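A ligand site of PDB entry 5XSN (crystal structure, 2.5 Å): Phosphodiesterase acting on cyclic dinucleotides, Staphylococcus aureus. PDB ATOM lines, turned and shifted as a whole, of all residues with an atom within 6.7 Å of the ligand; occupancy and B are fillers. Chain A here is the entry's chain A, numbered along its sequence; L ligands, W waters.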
ATOM      1  N   ARG A 187      13.298   6.385 -33.384  1.00  0.00           N
ATOM      2  CA  ARG A 187      13.517   7.780 -33.028  1.00  0.00           C
ATOM      3  C   ARG A 187      14.673   8.359 -33.806  1.00  0.00           C
ATOM      4  O   ARG A 187      15.725   8.632 -33.213  1.00  0.00           O
ATOM      5  CB  ARG A 187      13.810   7.959 -31.556  1.00  0.00           C
ATOM      6  CG  ARG A 187      13.117   6.927 -30.803  1.00  0.00           C
ATOM      7  CD  ARG A 187      12.222   7.516 -29.745  1.00  0.00           C
ATOM      8  NE  ARG A 187      12.069   6.496 -28.725  1.00  0.00           N
ATOM      9  CZ  ARG A 187      11.121   6.506 -27.799  1.00  0.00           C
ATOM     10  NH1 ARG A 187      10.222   7.459 -27.761  1.00  0.00           N
ATOM     11  NH2 ARG A 187      11.073   5.530 -26.907  1.00  0.00           N
ATOM     12  N   PRO A 255       1.096  12.390 -18.882  1.00  0.00           N
ATOM     13  CA  PRO A 255       2.102  11.308 -18.796  1.00  0.00           C
ATOM     14  C   PRO A 255       3.094  11.255 -19.957  1.00  0.00           C
ATOM     15  O   PRO A 255       4.238  10.809 -19.763  1.00  0.00           O
ATOM     16  CB  PRO A 255       1.228  10.042 -18.745  1.00  0.00           C
ATOM     17  CG  PRO A 255      -0.040  10.492 -18.097  1.00  0.00           C
ATOM     18  CD  PRO A 255      -0.262  11.912 -18.575  1.00  0.00           C
ATOM     19  N   VAL A 256       2.705  11.670 -21.166  1.00  0.00           N
ATOM     20  CA  VAL A 256       3.665  11.613 -22.265  1.00  0.00           C
ATOM     21  C   VAL A 256       4.664  12.754 -22.172  1.00  0.00           C
ATOM     22  O   VAL A 256       5.854  12.575 -22.438  1.00  0.00           O
ATOM     23  CB  VAL A 256       2.933  11.608 -23.624  1.00  0.00           C
ATOM     24  CG1 VAL A 256       3.936  11.698 -24.778  1.00  0.00           C
ATOM     25  CG2 VAL A 256       2.088  10.338 -23.768  1.00  0.00           C
ATOM     26  N   THR A 257       4.210  13.947 -21.768  1.00  0.00           N
ATOM     27  CA  THR A 257       5.106  15.062 -21.473  1.00  0.00           C
ATOM     28  C   THR A 257       6.204  14.673 -20.491  1.00  0.00           C
ATOM     29  O   THR A 257       7.374  15.045 -20.678  1.00  0.00           O
ATOM     30  CB  THR A 257       4.306  16.224 -20.908  1.00  0.00           C
ATOM     31  OG1 THR A 257       3.354  16.676 -21.884  1.00  0.00           O
ATOM     32  CG2 THR A 257       5.250  17.373 -20.486  1.00  0.00           C
ATOM     33  N   VAL A 258       5.844  13.958 -19.424  1.00  0.00           N
ATOM     34  CA  VAL A 258       6.835  13.459 -18.469  1.00  0.00           C
ATOM     35  C   VAL A 258       7.798  12.504 -19.163  1.00  0.00           C
ATOM     36  O   VAL A 258       9.019  12.614 -18.995  1.00  0.00           O
ATOM     37  CB  VAL A 258       6.149  12.781 -17.270  1.00  0.00           C
ATOM     38  CG1 VAL A 258       7.202  12.368 -16.250  1.00  0.00           C
ATOM     39  CG2 VAL A 258       5.115  13.700 -16.631  1.00  0.00           C
ATOM     40  N   ALA A 259       7.271  11.586 -19.954  1.00  0.00           N
ATOM     41  CA  ALA A 259       8.121  10.619 -20.635  1.00  0.00           C
ATOM     42  C   ALA A 259       9.065  11.300 -21.600  1.00  0.00           C
ATOM     43  O   ALA A 259      10.228  10.892 -21.756  1.00  0.00           O
ATOM     44  CB  ALA A 259       7.252   9.586 -21.375  1.00  0.00           C
ATOM     45  N   GLN A 260       8.583  12.339 -22.275  1.00  0.00           N
ATOM     46  CA  GLN A 260       9.392  13.069 -23.245  1.00  0.00           C
ATOM     47  C   GLN A 260      10.443  13.928 -22.547  1.00  0.00           C
ATOM     48  O   GLN A 260      11.562  14.052 -23.035  1.00  0.00           O
ATOM     49  CB  GLN A 260       8.472  13.927 -24.132  1.00  0.00           C
ATOM     50  CG  GLN A 260       7.748  13.106 -25.161  1.00  0.00           C
ATOM     51  CD  GLN A 260       6.677  13.868 -25.908  1.00  0.00           C
ATOM     52  OE1 GLN A 260       6.225  14.934 -25.468  1.00  0.00           O
ATOM     53  NE2 GLN A 260       6.252  13.319 -27.039  1.00  0.00           N
ATOM     54  N   ALA A 262      11.950  12.998 -19.871  1.00  0.00           N
ATOM     55  CA  ALA A 262      13.023  12.060 -19.526  1.00  0.00           C
ATOM     56  C   ALA A 262      13.826  11.680 -20.754  1.00  0.00           C
ATOM     57  O   ALA A 262      15.052  11.547 -20.664  1.00  0.00           O
ATOM     58  CB  ALA A 262      12.451  10.817 -18.850  1.00  0.00           C
ATOM     59  N   ASP A 263      13.170  11.508 -21.914  1.00  0.00           N
ATOM     60  CA  ASP A 263      13.895  11.198 -23.145  1.00  0.00           C
ATOM     61  C   ASP A 263      14.879  12.303 -23.477  1.00  0.00           C
ATOM     62  O   ASP A 263      16.055  12.047 -23.767  1.00  0.00           O
ATOM     63  CB  ASP A 263      12.948  11.008 -24.318  1.00  0.00           C
ATOM     64  CG  ASP A 263      12.123   9.749 -24.216  1.00  0.00           C
ATOM     65  OD1 ASP A 263      12.688   8.708 -23.799  1.00  0.00           O
ATOM     66  OD2 ASP A 263      10.913   9.828 -24.540  1.00  0.00           O
ATOM     67  N   ARG A 280       0.686  12.973 -11.522  1.00  0.00           N
ATOM     68  CA  ARG A 280      -0.166  12.478 -12.574  1.00  0.00           C
ATOM     69  C   ARG A 280      -1.646  12.568 -12.233  1.00  0.00           C
ATOM     70  O   ARG A 280      -2.458  12.775 -13.140  1.00  0.00           O
ATOM     71  CB  ARG A 280       0.191  11.019 -12.914  1.00  0.00           C
ATOM     72  CG  ARG A 280      -0.496  10.499 -14.172  1.00  0.00           C
ATOM     73  CD  ARG A 280      -0.443   8.981 -14.298  1.00  0.00           C
ATOM     74  NE  ARG A 280       0.799   8.506 -14.878  1.00  0.00           N
ATOM     75  CZ  ARG A 280       0.927   7.356 -15.537  1.00  0.00           C
ATOM     76  NH1 ARG A 280      -0.127   6.578 -15.698  1.00  0.00           N
ATOM     77  NH2 ARG A 280       2.096   6.993 -16.051  1.00  0.00           N
ATOM     78  N   ILE A 287       6.826   8.621 -12.308  1.00  0.00           N
ATOM     79  CA  ILE A 287       8.255   8.748 -12.533  1.00  0.00           C
ATOM     80  C   ILE A 287       8.578   8.057 -13.843  1.00  0.00           C
ATOM     81  O   ILE A 287       8.371   6.843 -13.961  1.00  0.00           O
ATOM     82  CB  ILE A 287       9.090   8.134 -11.401  1.00  0.00           C
ATOM     83  CG1 ILE A 287       8.658   8.709 -10.038  1.00  0.00           C
ATOM     84  CG2 ILE A 287      10.597   8.290 -11.725  1.00  0.00           C
ATOM     85  CD1 ILE A 287       9.404   8.133  -8.885  1.00  0.00           C
ATOM     86  N   SER A 288       9.127   8.799 -14.811  1.00  0.00           N
ATOM     87  CA  SER A 288       9.681   8.226 -16.026  1.00  0.00           C
ATOM     88  C   SER A 288      11.192   8.187 -15.929  1.00  0.00           C
ATOM     89  O   SER A 288      11.820   9.182 -15.535  1.00  0.00           O
ATOM     90  CB  SER A 288       9.254   9.015 -17.272  1.00  0.00           C
ATOM     91  OG  SER A 288       7.990   8.580 -17.726  1.00  0.00           O
ATOM     92  N   ALA A 289      11.790   7.036 -16.280  1.00  0.00           N
ATOM     93  CA  ALA A 289      13.231   6.867 -16.207  1.00  0.00           C
ATOM     94  C   ALA A 289      13.784   6.396 -17.544  1.00  0.00           C
ATOM     95  O   ALA A 289      13.135   5.636 -18.269  1.00  0.00           O
ATOM     96  CB  ALA A 289      13.628   5.881 -15.110  1.00  0.00           C
ATOM     97  N   ARG A 290      14.997   6.866 -17.867  1.00  0.00           N
ATOM     98  CA  ARG A 290      15.634   6.599 -19.147  1.00  0.00           C
ATOM     99  C   ARG A 290      17.138   6.598 -18.941  1.00  0.00           C
ATOM    100  O   ARG A 290      17.661   7.251 -18.028  1.00  0.00           O
ATOM    101  CB  ARG A 290      15.255   7.650 -20.212  1.00  0.00           C
ATOM    102  CG  ARG A 290      13.769   7.842 -20.473  1.00  0.00           C
ATOM    103  CD  ARG A 290      13.119   6.639 -21.162  1.00  0.00           C
ATOM    104  NE  ARG A 290      11.739   6.928 -21.541  1.00  0.00           N
ATOM    105  CZ  ARG A 290      10.689   6.761 -20.726  1.00  0.00           C
ATOM    106  NH1 ARG A 290      10.861   6.295 -19.499  1.00  0.00           N
ATOM    107  NH2 ARG A 290       9.460   7.048 -21.142  1.00  0.00           N
ATOM    108  N   GLY A 305       8.317  -0.502  -7.320  1.00  0.00           N
ATOM    109  CA  GLY A 305       7.040  -1.057  -7.695  1.00  0.00           C
ATOM    110  C   GLY A 305       6.641  -0.886  -9.155  1.00  0.00           C
ATOM    111  O   GLY A 305       5.469  -1.087  -9.474  1.00  0.00           O
ATOM    112  N   GLY A 306       7.579  -0.489 -10.021  1.00  0.00           N
ATOM    113  CA  GLY A 306       7.329  -0.410 -11.454  1.00  0.00           C
ATOM    114  C   GLY A 306       8.229  -1.361 -12.226  1.00  0.00           C
ATOM    115  O   GLY A 306       8.587  -2.425 -11.704  1.00  0.00           O
ATOM    116  N   GLY A 307       8.614  -0.996 -13.445  1.00  0.00           N
ATOM    117  CA  GLY A 307       9.562  -1.817 -14.183  1.00  0.00           C
ATOM    118  C   GLY A 307       9.724  -1.316 -15.611  1.00  0.00           C
ATOM    119  O   GLY A 307       9.478  -0.140 -15.901  1.00  0.00           O
ATOM    120  N   GLY A 308      10.144  -2.226 -16.488  1.00  0.00           N
ATOM    121  CA  GLY A 308      10.401  -1.903 -17.883  1.00  0.00           C
ATOM    122  C   GLY A 308      11.699  -2.508 -18.369  1.00  0.00           C
ATOM    123  O   GLY A 308      12.001  -3.665 -18.067  1.00  0.00           O
ATOM    124  N   HIS A 309      12.480  -1.748 -19.117  1.00  0.00           N
ATOM    125  CA  HIS A 309      13.694  -2.259 -19.724  1.00  0.00           C
ATOM    126  C   HIS A 309      14.888  -1.455 -19.236  1.00  0.00           C
ATOM    127  O   HIS A 309      14.738  -0.419 -18.589  1.00  0.00           O
ATOM    128  CB  HIS A 309      13.567  -2.245 -21.256  1.00  0.00           C
ATOM    129  CG  HIS A 309      12.291  -2.851 -21.743  1.00  0.00           C
ATOM    130  ND1 HIS A 309      12.082  -4.212 -21.787  1.00  0.00           N
ATOM    131  CD2 HIS A 309      11.130  -2.280 -22.156  1.00  0.00           C
ATOM    132  CE1 HIS A 309      10.857  -4.462 -22.226  1.00  0.00           C
ATOM    133  NE2 HIS A 309      10.253  -3.302 -22.444  1.00  0.00           N
ATOM    134  N   ASN A 312      14.669   2.099 -20.306  1.00  0.00           N
ATOM    135  CA  ASN A 312      13.332   2.664 -20.480  1.00  0.00           C
ATOM    136  C   ASN A 312      12.421   2.034 -19.436  1.00  0.00           C
ATOM    137  O   ASN A 312      12.028   0.869 -19.597  1.00  0.00           O
ATOM    138  CB  ASN A 312      12.825   2.396 -21.899  1.00  0.00           C
ATOM    139  CG  ASN A 312      11.416   2.933 -22.167  1.00  0.00           C
ATOM    140  OD1 ASN A 312      10.880   3.761 -21.413  1.00  0.00           O
ATOM    141  ND2 ASN A 312      10.818   2.474 -23.253  1.00  0.00           N
ATOM    142  N   ALA A 313      12.051   2.789 -18.406  1.00  0.00           N
ATOM    143  CA  ALA A 313      11.263   2.226 -17.313  1.00  0.00           C
ATOM    144  C   ALA A 313      10.421   3.322 -16.668  1.00  0.00           C
ATOM    145  O   ALA A 313      10.557   4.503 -16.982  1.00  0.00           O
ATOM    146  CB  ALA A 313      12.182   1.564 -16.275  1.00  0.00           C
ATOM    147  N   ALA A 314       9.550   2.914 -15.734  1.00  0.00           N
ATOM    148  CA  ALA A 314       8.708   3.855 -15.018  1.00  0.00           C
ATOM    149  C   ALA A 314       8.015   3.168 -13.840  1.00  0.00           C
ATOM    150  O   ALA A 314       8.078   1.948 -13.663  1.00  0.00           O
ATOM    151  CB  ALA A 314       7.661   4.506 -15.920  1.00  0.00           C
ATOM    152  N   THR A 315       7.361   3.995 -13.031  1.00  0.00           N
ATOM    153  CA  THR A 315       6.555   3.538 -11.906  1.00  0.00           C
ATOM    154  C   THR A 315       5.588   4.649 -11.548  1.00  0.00           C
ATOM    155  O   THR A 315       5.796   5.814 -11.920  1.00  0.00           O
ATOM    156  CB  THR A 315       7.395   3.194 -10.660  1.00  0.00           C
ATOM    157  OG1 THR A 315       6.541   2.588  -9.684  1.00  0.00           O
ATOM    158  CG2 THR A 315       8.011   4.468 -10.057  1.00  0.00           C
ATOM    159  N   GLN A 316       4.538   4.286 -10.834  1.00  0.00           N
ATOM    160  CA  GLN A 316       3.544   5.224 -10.315  1.00  0.00           C
ATOM    161  C   GLN A 316       3.386   4.970  -8.819  1.00  0.00           C
ATOM    162  O   GLN A 316       3.437   3.820  -8.373  1.00  0.00           O
ATOM    163  CB  GLN A 316       2.222   5.092 -11.075  1.00  0.00           C
ATOM    164  CG  GLN A 316       2.359   5.262 -12.627  1.00  0.00           C
ATOM    165  CD  GLN A 316       2.928   4.013 -13.333  1.00  0.00           C
ATOM    166  OE1 GLN A 316       2.560   2.882 -12.989  1.00  0.00           O
ATOM    167  NE2 GLN A 316       3.821   4.218 -14.296  1.00  0.00           N
HETATM  168  P1  LIG L   1       6.595   5.597 -19.254  1.00  0.00           P
HETATM  169  O1  LIG L   1       5.589   5.851 -18.247  1.00  0.00           O
HETATM  170  O2  LIG L   1       7.887   6.133 -19.128  1.00  0.00           O
HETATM  171  O3  LIG L   1       6.672   4.083 -19.513  1.00  0.00           O
HETATM  172  C1  LIG L   1       7.904   3.495 -19.778  1.00  0.00           C
HETATM  173  C2  LIG L   1       7.843   1.986 -19.785  1.00  0.00           C
HETATM  174  O4  LIG L   1       7.923   1.531 -18.460  1.00  0.00           O
HETATM  175  C3  LIG L   1       6.545   1.378 -20.251  1.00  0.00           C
HETATM  176  O5  LIG L   1       6.516   1.078 -21.614  1.00  0.00           O
HETATM  177  C4  LIG L   1       6.530   0.063 -19.549  1.00  0.00           C
HETATM  178  O6  LIG L   1       7.350  -0.754 -20.323  1.00  0.00           O
HETATM  179  C5  LIG L   1       7.233   0.331 -18.250  1.00  0.00           C
HETATM  180  N1  LIG L   1       6.311   0.608 -17.150  1.00  0.00           N
HETATM  181  C6  LIG L   1       5.686   1.736 -16.997  1.00  0.00           C
HETATM  182  N2  LIG L   1       4.950   1.735 -15.907  1.00  0.00           N
HETATM  183  C7  LIG L   1       5.091   0.587 -15.312  1.00  0.00           C
HETATM  184  C8  LIG L   1       4.562  -0.060 -14.092  1.00  0.00           C
HETATM  185  N3  LIG L   1       3.742   0.545 -13.238  1.00  0.00           N
HETATM  186  N4  LIG L   1       4.963  -1.280 -13.836  1.00  0.00           N
HETATM  187  C9  LIG L   1       5.808  -1.899 -14.633  1.00  0.00           C
HETATM  188  N5  LIG L   1       6.319  -1.390 -15.747  1.00  0.00           N
HETATM  189  C10 LIG L   1       6.001  -0.154 -16.135  1.00  0.00           C
HETATM  190  P2  LIG L   1       5.174   1.269 -22.391  1.00  0.00           P
HETATM  191  O7  LIG L   1       5.638   1.162 -23.756  1.00  0.00           O
HETATM  192  O8  LIG L   1       4.145   0.390 -21.870  1.00  0.00           O
HETATM  193  O9  LIG L   1       4.632   2.677 -22.033  1.00  0.00           O
HETATM  194  C11 LIG L   1       4.743   3.716 -22.955  1.00  0.00           C
HETATM  195  C12 LIG L   1       5.699   4.730 -22.387  1.00  0.00           C
HETATM  196  O10 LIG L   1       6.042   5.637 -23.415  1.00  0.00           O
HETATM  197  C13 LIG L   1       5.027   5.556 -21.342  1.00  0.00           C
HETATM  198  O11 LIG L   1       6.021   6.182 -20.565  1.00  0.00           O
HETATM  199  C14 LIG L   1       4.413   6.646 -22.124  1.00  0.00           C
HETATM  200  O12 LIG L   1       4.218   7.695 -21.208  1.00  0.00           O
HETATM  201  C15 LIG L   1       5.501   6.903 -23.147  1.00  0.00           C
HETATM  202  N6  LIG L   1       4.971   7.448 -24.396  1.00  0.00           N
HETATM  203  C16 LIG L   1       3.756   7.233 -24.880  1.00  0.00           C
HETATM  204  N7  LIG L   1       3.577   7.886 -26.030  1.00  0.00           N
HETATM  205  C17 LIG L   1       4.712   8.538 -26.314  1.00  0.00           C
HETATM  206  C18 LIG L   1       5.210   9.432 -27.372  1.00  0.00           C
HETATM  207  N8  LIG L   1       4.455   9.786 -28.415  1.00  0.00           N
HETATM  208  N9  LIG L   1       6.462   9.903 -27.267  1.00  0.00           N
HETATM  209  C19 LIG L   1       7.230   9.602 -26.245  1.00  0.00           C
HETATM  210  N10 LIG L   1       6.841   8.797 -25.266  1.00  0.00           N
HETATM  211  C20 LIG L   1       5.622   8.252 -25.222  1.00  0.00           C
HETATM  212  O   HOH W   1       9.246   7.920 -24.012  1.00  0.00           O
HETATM  213  O   HOH W   2       3.990  -2.758 -10.886  1.00  0.00           O
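The backbone NH (N) of Ala 314 is in hydrogen-bond range of an oxygen (O4) of the ligand, at 3.5 Å.
The side-chain hydroxyl (OG) of Ser 288 lies within hydrogen-bond range of an oxygen (O2) of the ligand, at 2.8 Å.
A nitrogen (N9) of the ligand sits at hydrogen-bond distance from the side-chain amide nitrogen (NE2) of Gln 260, 3.4 Å away.
N of Gly 307 lies close to N5 of the ligand (3.3 Å).
O2 of the ligand is in salt-bridge range of NH2 of Arg 290, at 2.7 Å.
OE1 of Gln 316 sits at hydrogen-bond distance from N3 of the ligand (2.6 Å).
The backbone carbonyl oxygen (O) of Pro 255 is in hydrogen-bond range of an oxygen (O12) of the ligand.
OG1 of Thr 315 sits at hydrogen-bond distance from N of Gly 306 (3.3 Å).
NE of Arg 290 is in salt-bridge range of OD1 of Asp 263 (3.0 Å).
The guanidinium group (NH1) of Arg 290 lies within hydrogen-bond range of the backbone carbonyl oxygen (O) of Ala 313.
O of Ala 313 lies within hydrogen-bond range of N of Ala 289, at 2.9 Å.
The guanidinium group of Arg 290 lies close to the side-chain amide oxygen of Asn 312 (3.2 Å).
N of Gly 307 sits at hydrogen-bond distance from O of Ala 314.
Arg 187 touches the ligand (NH1 to C19, 3.98 Å).
Val 256 touches the ligand.
Ala 259 touches the ligand (CB to O12, 3.6 Å).
C of Gly 306 touches C9 of the ligand, at 3.5 Å.
CA of Gly 308 touches C5 of the ligand, at 3.9 Å.
Asn 312 touches the ligand (OD1 to C1, 3.4 Å).
Ala 313 touches the ligand (C to O4, 3.6 Å).
Of the 24 residues printed, 14 come within 4 Å of the ligand.
The nearest printed residue that does not touch the ligand is Asp 263 (4.1 Å).
Water W1 lies within hydrogen-bond range of the side-chain carboxylate of Asp 263 (2.6 Å), a nitrogen (N10) of the ligand (2.9 Å) and the guanidinium group of Arg 290 (3.0 Å).
Water W2 bridges O of Gly 305 and N4 of the ligand.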
